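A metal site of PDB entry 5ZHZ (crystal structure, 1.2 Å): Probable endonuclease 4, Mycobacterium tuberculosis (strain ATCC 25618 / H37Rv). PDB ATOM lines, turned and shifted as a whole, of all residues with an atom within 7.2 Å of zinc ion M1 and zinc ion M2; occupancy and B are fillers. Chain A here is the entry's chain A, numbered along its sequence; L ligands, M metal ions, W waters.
OE1 of Gln 25 is in hydrogen-bond range of NE2 of His 191 (2.8 Å).
A ring nitrogen (ND1) of His 165 lies within hydrogen-bond range of the backbone carbonyl oxygen of Asn 130, 2.8 Å away.
OD1 of Asp 162 sits at hydrogen-bond distance from N of Cys 164.
A ring nitrogen (NE2) of His 191 is in hydrogen-bond range of the side-chain sulfur (SG) of Cys 160, at 3.4 Å.
The backbone NH (N) of Asp 162 sits at hydrogen-bond distance from the side-chain amide oxygen (OD1) of Asn 130 (2.9 Å).
The backbone NH (N) of Glu 233 sits at hydrogen-bond distance from the side-chain amide oxygen (OD1) of Asn 193 (2.7 Å).
The backbone carbonyl oxygen (O) of Leu 161 lies within hydrogen-bond range of the backbone NH (N) of His 191.
OE2 of Glu 233 sits at hydrogen-bond distance from NE2 of Gln 25, at 2.9 Å.
His 165 touches zinc ion M1 (CE1 to ZN, 3.8 Å).
Five residues have an atom within 4 Å of zinc ion M1: Glu 129, Asp 162, His 165, His 191 and Glu 233.
Along chain A the residues within 4 Å of zinc ion M1 span positions 129 to 233.
The nearest printed residue that does not touch zinc ion M1 is Asn 193 (4.1 Å).
Three residues have an atom within 4 Å of zinc ion M2: His 56, His 96 and Glu 129.
Along chain A the residues within 4 Å of zinc ion M2 span positions 56 to 129.
Zinc ion M1 is bound by OD2 of Asp 162 (2.1 Å), OE2 of Glu 129 (2.1 Å), water W1 (2.1 Å), OE1 of Glu 233 (2.1 Å), O2 of the ligand (2.2 Å) and ND1 of His 191 (2.2 Å).
Zinc ion M1 has six donor atoms within binding distance.
Zinc ion M2 is bound by a ring nitrogen (NE2) of His 96, 2.0 Å away.
Water W1 is bound to zinc ion M2 (2.0 Å).
OE1 of Glu 129 binds zinc ion M2 (2.0 Å).
Zinc ion M2 is bound by a ring nitrogen (NE2) of His 56 (2.1 Å).
An oxygen (O3) of the ligand binds zinc ion M2, 2.1 Å away.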
ATOM      1  N   GLN A  25      11.818 -24.233  16.614  1.00  0.00           N
ATOM      2  CA  GLN A  25      11.510 -22.912  16.095  1.00  0.00           C
ATOM      3  C   GLN A  25      12.734 -22.431  15.310  1.00  0.00           C
ATOM      4  O   GLN A  25      13.875 -22.675  15.730  1.00  0.00           O
ATOM      5  CB  GLN A  25      11.203 -21.970  17.241  1.00  0.00           C
ATOM      6  CG  GLN A  25      10.759 -20.567  16.831  1.00  0.00           C
ATOM      7  CD  GLN A  25      10.493 -19.744  18.051  1.00  0.00           C
ATOM      8  OE1 GLN A  25       9.349 -19.701  18.564  1.00  0.00           O
ATOM      9  NE2 GLN A  25      11.541 -19.106  18.596  1.00  0.00           N
ATOM     10  N   PHE A  27      14.232 -19.146  12.424  1.00  0.00           N
ATOM     11  CA  PHE A  27      14.084 -18.022  11.505  1.00  0.00           C
ATOM     12  C   PHE A  27      14.219 -18.514  10.084  1.00  0.00           C
ATOM     13  O   PHE A  27      14.948 -19.455   9.774  1.00  0.00           O
ATOM     14  CB  PHE A  27      15.161 -16.959  11.748  1.00  0.00           C
ATOM     15  CG  PHE A  27      14.972 -16.182  13.040  1.00  0.00           C
ATOM     16  CD1 PHE A  27      14.183 -15.039  13.025  1.00  0.00           C
ATOM     17  CD2 PHE A  27      15.519 -16.604  14.224  1.00  0.00           C
ATOM     18  CE1 PHE A  27      13.986 -14.290  14.167  1.00  0.00           C
ATOM     19  CE2 PHE A  27      15.296 -15.821  15.391  1.00  0.00           C
ATOM     20  CZ  PHE A  27      14.521 -14.710  15.340  1.00  0.00           C
ATOM     21  N   HIS A  56       9.928 -17.838  13.744  1.00  0.00           N
ATOM     22  CA  HIS A  56      10.055 -16.525  14.345  1.00  0.00           C
ATOM     23  C   HIS A  56      10.184 -15.470  13.260  1.00  0.00           C
ATOM     24  O   HIS A  56      11.054 -15.596  12.390  1.00  0.00           O
ATOM     25  CB  HIS A  56      11.281 -16.498  15.280  1.00  0.00           C
ATOM     26  CG  HIS A  56      11.243 -15.404  16.302  1.00  0.00           C
ATOM     27  ND1 HIS A  56      11.088 -14.059  15.981  1.00  0.00           N
ATOM     28  CD2 HIS A  56      11.315 -15.453  17.657  1.00  0.00           C
ATOM     29  CE1 HIS A  56      11.059 -13.358  17.105  1.00  0.00           C
ATOM     30  NE2 HIS A  56      11.213 -14.167  18.143  1.00  0.00           N
ATOM     31  N   ALA A  57       9.317 -14.461  13.267  1.00  0.00           N
ATOM     32  CA  ALA A  57       9.411 -13.401  12.289  1.00  0.00           C
ATOM     33  C   ALA A  57      10.635 -12.521  12.593  1.00  0.00           C
ATOM     34  O   ALA A  57      11.062 -12.432  13.745  1.00  0.00           O
ATOM     35  CB  ALA A  57       8.148 -12.545  12.343  1.00  0.00           C
ATOM     36  N   TYR A  59      13.298  -9.796  13.687  1.00  0.00           N
ATOM     37  CA  TYR A  59      13.266  -8.975  14.893  1.00  0.00           C
ATOM     38  C   TYR A  59      12.944  -7.516  14.625  1.00  0.00           C
ATOM     39  O   TYR A  59      12.441  -6.830  15.525  1.00  0.00           O
ATOM     40  CB  TYR A  59      14.637  -8.971  15.513  1.00  0.00           C
ATOM     41  CG  TYR A  59      14.971 -10.226  16.262  1.00  0.00           C
ATOM     42  CD1 TYR A  59      14.067 -10.781  17.210  1.00  0.00           C
ATOM     43  CD2 TYR A  59      16.179 -10.885  16.065  1.00  0.00           C
ATOM     44  CE1 TYR A  59      14.396 -11.921  17.940  1.00  0.00           C
ATOM     45  CE2 TYR A  59      16.483 -12.042  16.793  1.00  0.00           C
ATOM     46  CZ  TYR A  59      15.616 -12.525  17.731  1.00  0.00           C
ATOM     47  OH  TYR A  59      15.965 -13.657  18.421  1.00  0.00           O
ATOM     48  N   ILE A  94       5.731 -16.303  15.109  1.00  0.00           N
ATOM     49  CA  ILE A  94       5.852 -15.511  16.324  1.00  0.00           C
ATOM     50  C   ILE A  94       6.416 -14.145  15.962  1.00  0.00           C
ATOM     51  O   ILE A  94       7.415 -14.050  15.250  1.00  0.00           O
ATOM     52  CB  ILE A  94       6.788 -16.232  17.323  1.00  0.00           C
ATOM     53  CG1 ILE A  94       6.199 -17.557  17.821  1.00  0.00           C
ATOM     54  CG2 ILE A  94       7.017 -15.351  18.554  1.00  0.00           C
ATOM     55  CD1 ILE A  94       6.301 -18.694  16.869  1.00  0.00           C
ATOM     56  N   VAL A  95       5.798 -13.085  16.477  1.00  0.00           N
ATOM     57  CA  VAL A  95       6.277 -11.727  16.206  1.00  0.00           C
ATOM     58  C   VAL A  95       6.290 -10.945  17.511  1.00  0.00           C
ATOM     59  O   VAL A  95       5.376 -11.051  18.334  1.00  0.00           O
ATOM     60  CB  VAL A  95       5.416 -11.053  15.119  1.00  0.00           C
ATOM     61  CG1 VAL A  95       4.024 -10.925  15.536  1.00  0.00           C
ATOM     62  CG2 VAL A  95       5.958  -9.691  14.754  1.00  0.00           C
ATOM     63  N   HIS A  96       7.328 -10.158  17.720  1.00  0.00           N
ATOM     64  CA  HIS A  96       7.434  -9.342  18.912  1.00  0.00           C
ATOM     65  C   HIS A  96       6.410  -8.210  18.911  1.00  0.00           C
ATOM     66  O   HIS A  96       5.950  -7.733  17.864  1.00  0.00           O
ATOM     67  CB  HIS A  96       8.856  -8.841  19.045  1.00  0.00           C
ATOM     68  CG  HIS A  96       9.870  -9.992  19.440  1.00  0.00           C
ATOM     69  ND1 HIS A  96      11.083  -9.545  19.836  1.00  0.00           N
ATOM     70  CD2 HIS A  96       9.964 -11.465  19.602  1.00  0.00           C
ATOM     71  CE1 HIS A  96      11.814 -10.613  20.121  1.00  0.00           C
ATOM     72  NE2 HIS A  96      11.121 -11.713  20.005  1.00  0.00           N
ATOM     73  N   GLU A 129       4.649 -12.010  20.958  1.00  0.00           N
ATOM     74  CA  GLU A 129       5.544 -12.329  22.063  1.00  0.00           C
ATOM     75  C   GLU A 129       5.875 -11.065  22.873  1.00  0.00           C
ATOM     76  O   GLU A 129       6.157  -9.996  22.309  1.00  0.00           O
ATOM     77  CB  GLU A 129       6.861 -12.935  21.491  1.00  0.00           C
ATOM     78  CG  GLU A 129       7.821 -13.418  22.586  1.00  0.00           C
ATOM     79  CD  GLU A 129       9.204 -13.845  22.089  1.00  0.00           C
ATOM     80  OE1 GLU A 129       9.365 -13.914  20.841  1.00  0.00           O
ATOM     81  OE2 GLU A 129      10.104 -14.078  22.936  1.00  0.00           O
ATOM     82  N   ASN A 130       5.874 -11.216  24.196  1.00  0.00           N
ATOM     83  CA  ASN A 130       6.316 -10.135  25.072  1.00  0.00           C
ATOM     84  C   ASN A 130       7.812  -9.894  24.931  1.00  0.00           C
ATOM     85  O   ASN A 130       8.571 -10.801  24.551  1.00  0.00           O
ATOM     86  CB  ASN A 130       5.948 -10.383  26.523  1.00  0.00           C
ATOM     87  CG  ASN A 130       6.573 -11.638  27.093  1.00  0.00           C
ATOM     88  OD1 ASN A 130       6.430 -12.722  26.543  1.00  0.00           O
ATOM     89  ND2 ASN A 130       7.211 -11.502  28.245  1.00  0.00           N
ATOM     90  N   THR A 131       8.249  -8.674  25.302  1.00  0.00           N
ATOM     91  CA  THR A 131       9.627  -8.234  25.072  1.00  0.00           C
ATOM     92  C   THR A 131      10.289  -7.793  26.365  1.00  0.00           C
ATOM     93  O   THR A 131       9.652  -7.594  27.388  1.00  0.00           O
ATOM     94  CB  THR A 131       9.634  -7.111  24.018  1.00  0.00           C
ATOM     95  OG1 THR A 131       8.773  -6.044  24.455  1.00  0.00           O
ATOM     96  CG2 THR A 131       9.146  -7.625  22.670  1.00  0.00           C
ATOM     97  N   CYS A 160       2.624 -15.628  22.901  1.00  0.00           N
ATOM     98  CA  CYS A 160       3.780 -16.404  23.283  1.00  0.00           C
ATOM     99  C   CYS A 160       4.439 -15.736  24.477  1.00  0.00           C
ATOM    100  O   CYS A 160       4.852 -14.565  24.395  1.00  0.00           O
ATOM    101  CB  CYS A 160       4.778 -16.441  22.107  1.00  0.00           C
ATOM    102  SG  CYS A 160       6.351 -17.207  22.535  1.00  0.00           S
ATOM    103  N   LEU A 161       4.533 -16.464  25.593  1.00  0.00           N
ATOM    104  CA  LEU A 161       5.155 -15.940  26.805  1.00  0.00           C
ATOM    105  C   LEU A 161       6.625 -16.346  26.851  1.00  0.00           C
ATOM    106  O   LEU A 161       6.942 -17.546  26.847  1.00  0.00           O
ATOM    107  CB  LEU A 161       4.420 -16.482  28.044  1.00  0.00           C
ATOM    108  CG  LEU A 161       5.029 -15.964  29.356  1.00  0.00           C
ATOM    109  CD1 LEU A 161       4.829 -14.439  29.530  1.00  0.00           C
ATOM    110  CD2 LEU A 161       4.399 -16.658  30.568  1.00  0.00           C
ATOM    111  N   ASP A 162       7.532 -15.356  26.899  1.00  0.00           N
ATOM    112  CA  ASP A 162       8.953 -15.626  27.020  1.00  0.00           C
ATOM    113  C   ASP A 162       9.357 -15.336  28.467  1.00  0.00           C
ATOM    114  O   ASP A 162       9.166 -14.205  28.975  1.00  0.00           O
ATOM    115  CB  ASP A 162       9.728 -14.775  26.024  1.00  0.00           C
ATOM    116  CG  ASP A 162      11.233 -15.120  25.999  1.00  0.00           C
ATOM    117  OD1 ASP A 162      11.843 -15.061  27.093  1.00  0.00           O
ATOM    118  OD2 ASP A 162      11.743 -15.428  24.910  1.00  0.00           O
ATOM    119  N   THR A 163       9.879 -16.364  29.149  1.00  0.00           N
ATOM    120  CA  THR A 163      10.198 -16.211  30.567  1.00  0.00           C
ATOM    121  C   THR A 163      11.380 -15.283  30.812  1.00  0.00           C
ATOM    122  O   THR A 163      11.423 -14.628  31.867  1.00  0.00           O
ATOM    123  CB  THR A 163      10.474 -17.568  31.226  1.00  0.00           C
ATOM    124  OG1 THR A 163      11.536 -18.233  30.519  1.00  0.00           O
ATOM    125  CG2 THR A 163       9.231 -18.475  31.144  1.00  0.00           C
ATOM    126  N   CYS A 164      12.372 -15.268  29.924  1.00  0.00           N
ATOM    127  CA  CYS A 164      13.477 -14.329  30.110  1.00  0.00           C
ATOM    128  C   CYS A 164      12.973 -12.900  29.974  1.00  0.00           C
ATOM    129  O   CYS A 164      13.365 -12.002  30.748  1.00  0.00           O
ATOM    130  CB  CYS A 164      14.607 -14.627  29.110  1.00  0.00           C
ATOM    131  SG  CYS A 164      16.066 -13.511  29.272  1.00  0.00           S
ATOM    132  N   HIS A 165      12.114 -12.660  28.990  1.00  0.00           N
ATOM    133  CA  HIS A 165      11.588 -11.317  28.788  1.00  0.00           C
ATOM    134  C   HIS A 165      10.778 -10.867  29.995  1.00  0.00           C
ATOM    135  O   HIS A 165      10.889  -9.710  30.444  1.00  0.00           O
ATOM    136  CB  HIS A 165      10.796 -11.216  27.480  1.00  0.00           C
ATOM    137  CG  HIS A 165      11.636 -11.570  26.290  1.00  0.00           C
ATOM    138  ND1 HIS A 165      11.170 -11.645  25.001  1.00  0.00           N
ATOM    139  CD2 HIS A 165      12.972 -11.878  26.223  1.00  0.00           C
ATOM    140  CE1 HIS A 165      12.158 -12.035  24.194  1.00  0.00           C
ATOM    141  NE2 HIS A 165      13.271 -12.179  24.917  1.00  0.00           N
ATOM    142  N   VAL A 190       5.254 -21.222  24.926  1.00  0.00           N
ATOM    143  CA  VAL A 190       6.158 -20.647  25.934  1.00  0.00           C
ATOM    144  C   VAL A 190       7.574 -20.713  25.413  1.00  0.00           C
ATOM    145  O   VAL A 190       7.988 -21.779  24.895  1.00  0.00           O
ATOM    146  CB  VAL A 190       6.019 -21.376  27.285  1.00  0.00           C
ATOM    147  CG1 VAL A 190       7.130 -21.009  28.241  1.00  0.00           C
ATOM    148  CG2 VAL A 190       4.672 -21.065  27.896  1.00  0.00           C
ATOM    149  N   HIS A 191       8.303 -19.613  25.533  1.00  0.00           N
ATOM    150  CA  HIS A 191       9.747 -19.624  25.335  1.00  0.00           C
ATOM    151  C   HIS A 191      10.346 -19.735  26.723  1.00  0.00           C
ATOM    152  O   HIS A 191      10.251 -18.786  27.529  1.00  0.00           O
ATOM    153  CB  HIS A 191      10.206 -18.343  24.654  1.00  0.00           C
ATOM    154  CG  HIS A 191       9.826 -18.248  23.221  1.00  0.00           C
ATOM    155  ND1 HIS A 191      10.038 -17.096  22.471  1.00  0.00           N
ATOM    156  CD2 HIS A 191       9.256 -19.164  22.398  1.00  0.00           C
ATOM    157  CE1 HIS A 191       9.637 -17.340  21.233  1.00  0.00           C
ATOM    158  NE2 HIS A 191       9.160 -18.580  21.152  1.00  0.00           N
ATOM    159  N   CYS A 192      10.912 -20.899  27.037  1.00  0.00           N
ATOM    160  CA  CYS A 192      11.426 -21.162  28.367  1.00  0.00           C
ATOM    161  C   CYS A 192      12.937 -20.937  28.370  1.00  0.00           C
ATOM    162  O   CYS A 192      13.724 -21.834  28.013  1.00  0.00           O
ATOM    163  CB  CYS A 192      11.079 -22.570  28.839  1.00  0.00           C
ATOM    164  SG  CYS A 192      11.554 -22.847  30.569  1.00  0.00           S
ATOM    165  N   ASN A 193      13.314 -19.739  28.786  1.00  0.00           N
ATOM    166  CA  ASN A 193      14.693 -19.237  28.804  1.00  0.00           C
ATOM    167  C   ASN A 193      15.067 -18.792  30.205  1.00  0.00           C
ATOM    168  O   ASN A 193      14.289 -18.111  30.863  1.00  0.00           O
ATOM    169  CB  ASN A 193      14.774 -18.019  27.873  1.00  0.00           C
ATOM    170  CG  ASN A 193      14.407 -18.351  26.463  1.00  0.00           C
ATOM    171  OD1 ASN A 193      14.785 -19.416  25.951  1.00  0.00           O
ATOM    172  ND2 ASN A 193      13.647 -17.456  25.815  1.00  0.00           N
ATOM    173  N   ASP A 204      18.374  -8.514  27.438  1.00  0.00           N
ATOM    174  CA  ASP A 204      17.827  -9.772  26.907  1.00  0.00           C
ATOM    175  C   ASP A 204      18.975 -10.700  26.572  1.00  0.00           C
ATOM    176  O   ASP A 204      19.441 -10.744  25.407  1.00  0.00           O
ATOM    177  CB  ASP A 204      17.008  -9.558  25.738  1.00  0.00           C
ATOM    178  CG  ASP A 204      16.351 -10.896  25.331  1.00  0.00           C
ATOM    179  OD1 ASP A 204      15.961 -11.661  26.212  1.00  0.00           O
ATOM    180  OD2 ASP A 204      16.163 -11.190  24.171  1.00  0.00           O
ATOM    181  N   HIS A 206      19.742 -14.548  27.022  1.00  0.00           N
ATOM    182  CA  HIS A 206      19.223 -15.845  27.466  1.00  0.00           C
ATOM    183  C   HIS A 206      20.343 -16.675  28.059  1.00  0.00           C
ATOM    184  O   HIS A 206      21.517 -16.512  27.726  1.00  0.00           O
ATOM    185  CB  HIS A 206      18.603 -16.606  26.292  1.00  0.00           C
ATOM    186  CG  HIS A 206      17.471 -15.874  25.594  1.00  0.00           C
ATOM    187  ND1 HIS A 206      16.761 -16.464  24.579  1.00  0.00           N
ATOM    188  CD2 HIS A 206      16.939 -14.620  25.720  1.00  0.00           C
ATOM    189  CE1 HIS A 206      15.842 -15.622  24.128  1.00  0.00           C
ATOM    190  NE2 HIS A 206      15.918 -14.469  24.796  1.00  0.00           N
ATOM    191  N   ILE A 231       9.508 -23.856  23.681  1.00  0.00           N
ATOM    192  CA  ILE A 231      10.754 -23.657  22.950  1.00  0.00           C
ATOM    193  C   ILE A 231      11.796 -23.139  23.927  1.00  0.00           C
ATOM    194  O   ILE A 231      11.623 -22.058  24.511  1.00  0.00           O
ATOM    195  CB  ILE A 231      10.600 -22.630  21.825  1.00  0.00           C
ATOM    196  CG1 ILE A 231       9.395 -22.832  20.926  1.00  0.00           C
ATOM    197  CG2 ILE A 231      11.897 -22.500  21.044  1.00  0.00           C
ATOM    198  CD1 ILE A 231       9.358 -24.078  20.280  1.00  0.00           C
ATOM    199  N   GLU A 233      15.109 -21.260  23.938  1.00  0.00           N
ATOM    200  CA  GLU A 233      15.873 -20.417  23.022  1.00  0.00           C
ATOM    201  C   GLU A 233      17.230 -20.129  23.649  1.00  0.00           C
ATOM    202  O   GLU A 233      17.665 -18.996  23.854  1.00  0.00           O
ATOM    203  CB  GLU A 233      15.130 -19.102  22.727  1.00  0.00           C
ATOM    204  CG  GLU A 233      13.722 -19.309  22.219  1.00  0.00           C
ATOM    205  CD  GLU A 233      13.033 -18.008  21.992  1.00  0.00           C
ATOM    206  OE1 GLU A 233      12.874 -17.227  22.944  1.00  0.00           O
ATOM    207  OE2 GLU A 233      12.699 -17.705  20.841  1.00  0.00           O
HETATM  208  S1  LIG L   1      14.050 -13.790  21.605  1.00  0.00           S
HETATM  209  O1  LIG L   1      14.828 -14.739  20.787  1.00  0.00           O
HETATM  210  O2  LIG L   1      13.391 -14.437  22.781  1.00  0.00           O
HETATM  211  O3  LIG L   1      13.108 -12.990  20.822  1.00  0.00           O
HETATM  212  O4  LIG L   1      14.985 -12.822  22.254  1.00  0.00           O
HETATM  213 ZN    ZN M   1      11.545 -15.560  22.858  1.00  0.00          ZN
HETATM  214 ZN    ZN M   2      11.225 -13.657  20.144  1.00  0.00          ZN
HETATM  215 ZN    ZN M   3      15.012 -12.807  24.224  1.00  0.00          ZN
HETATM  216  O   HOH W   1      11.714 -15.460  20.771  1.00  0.00           O
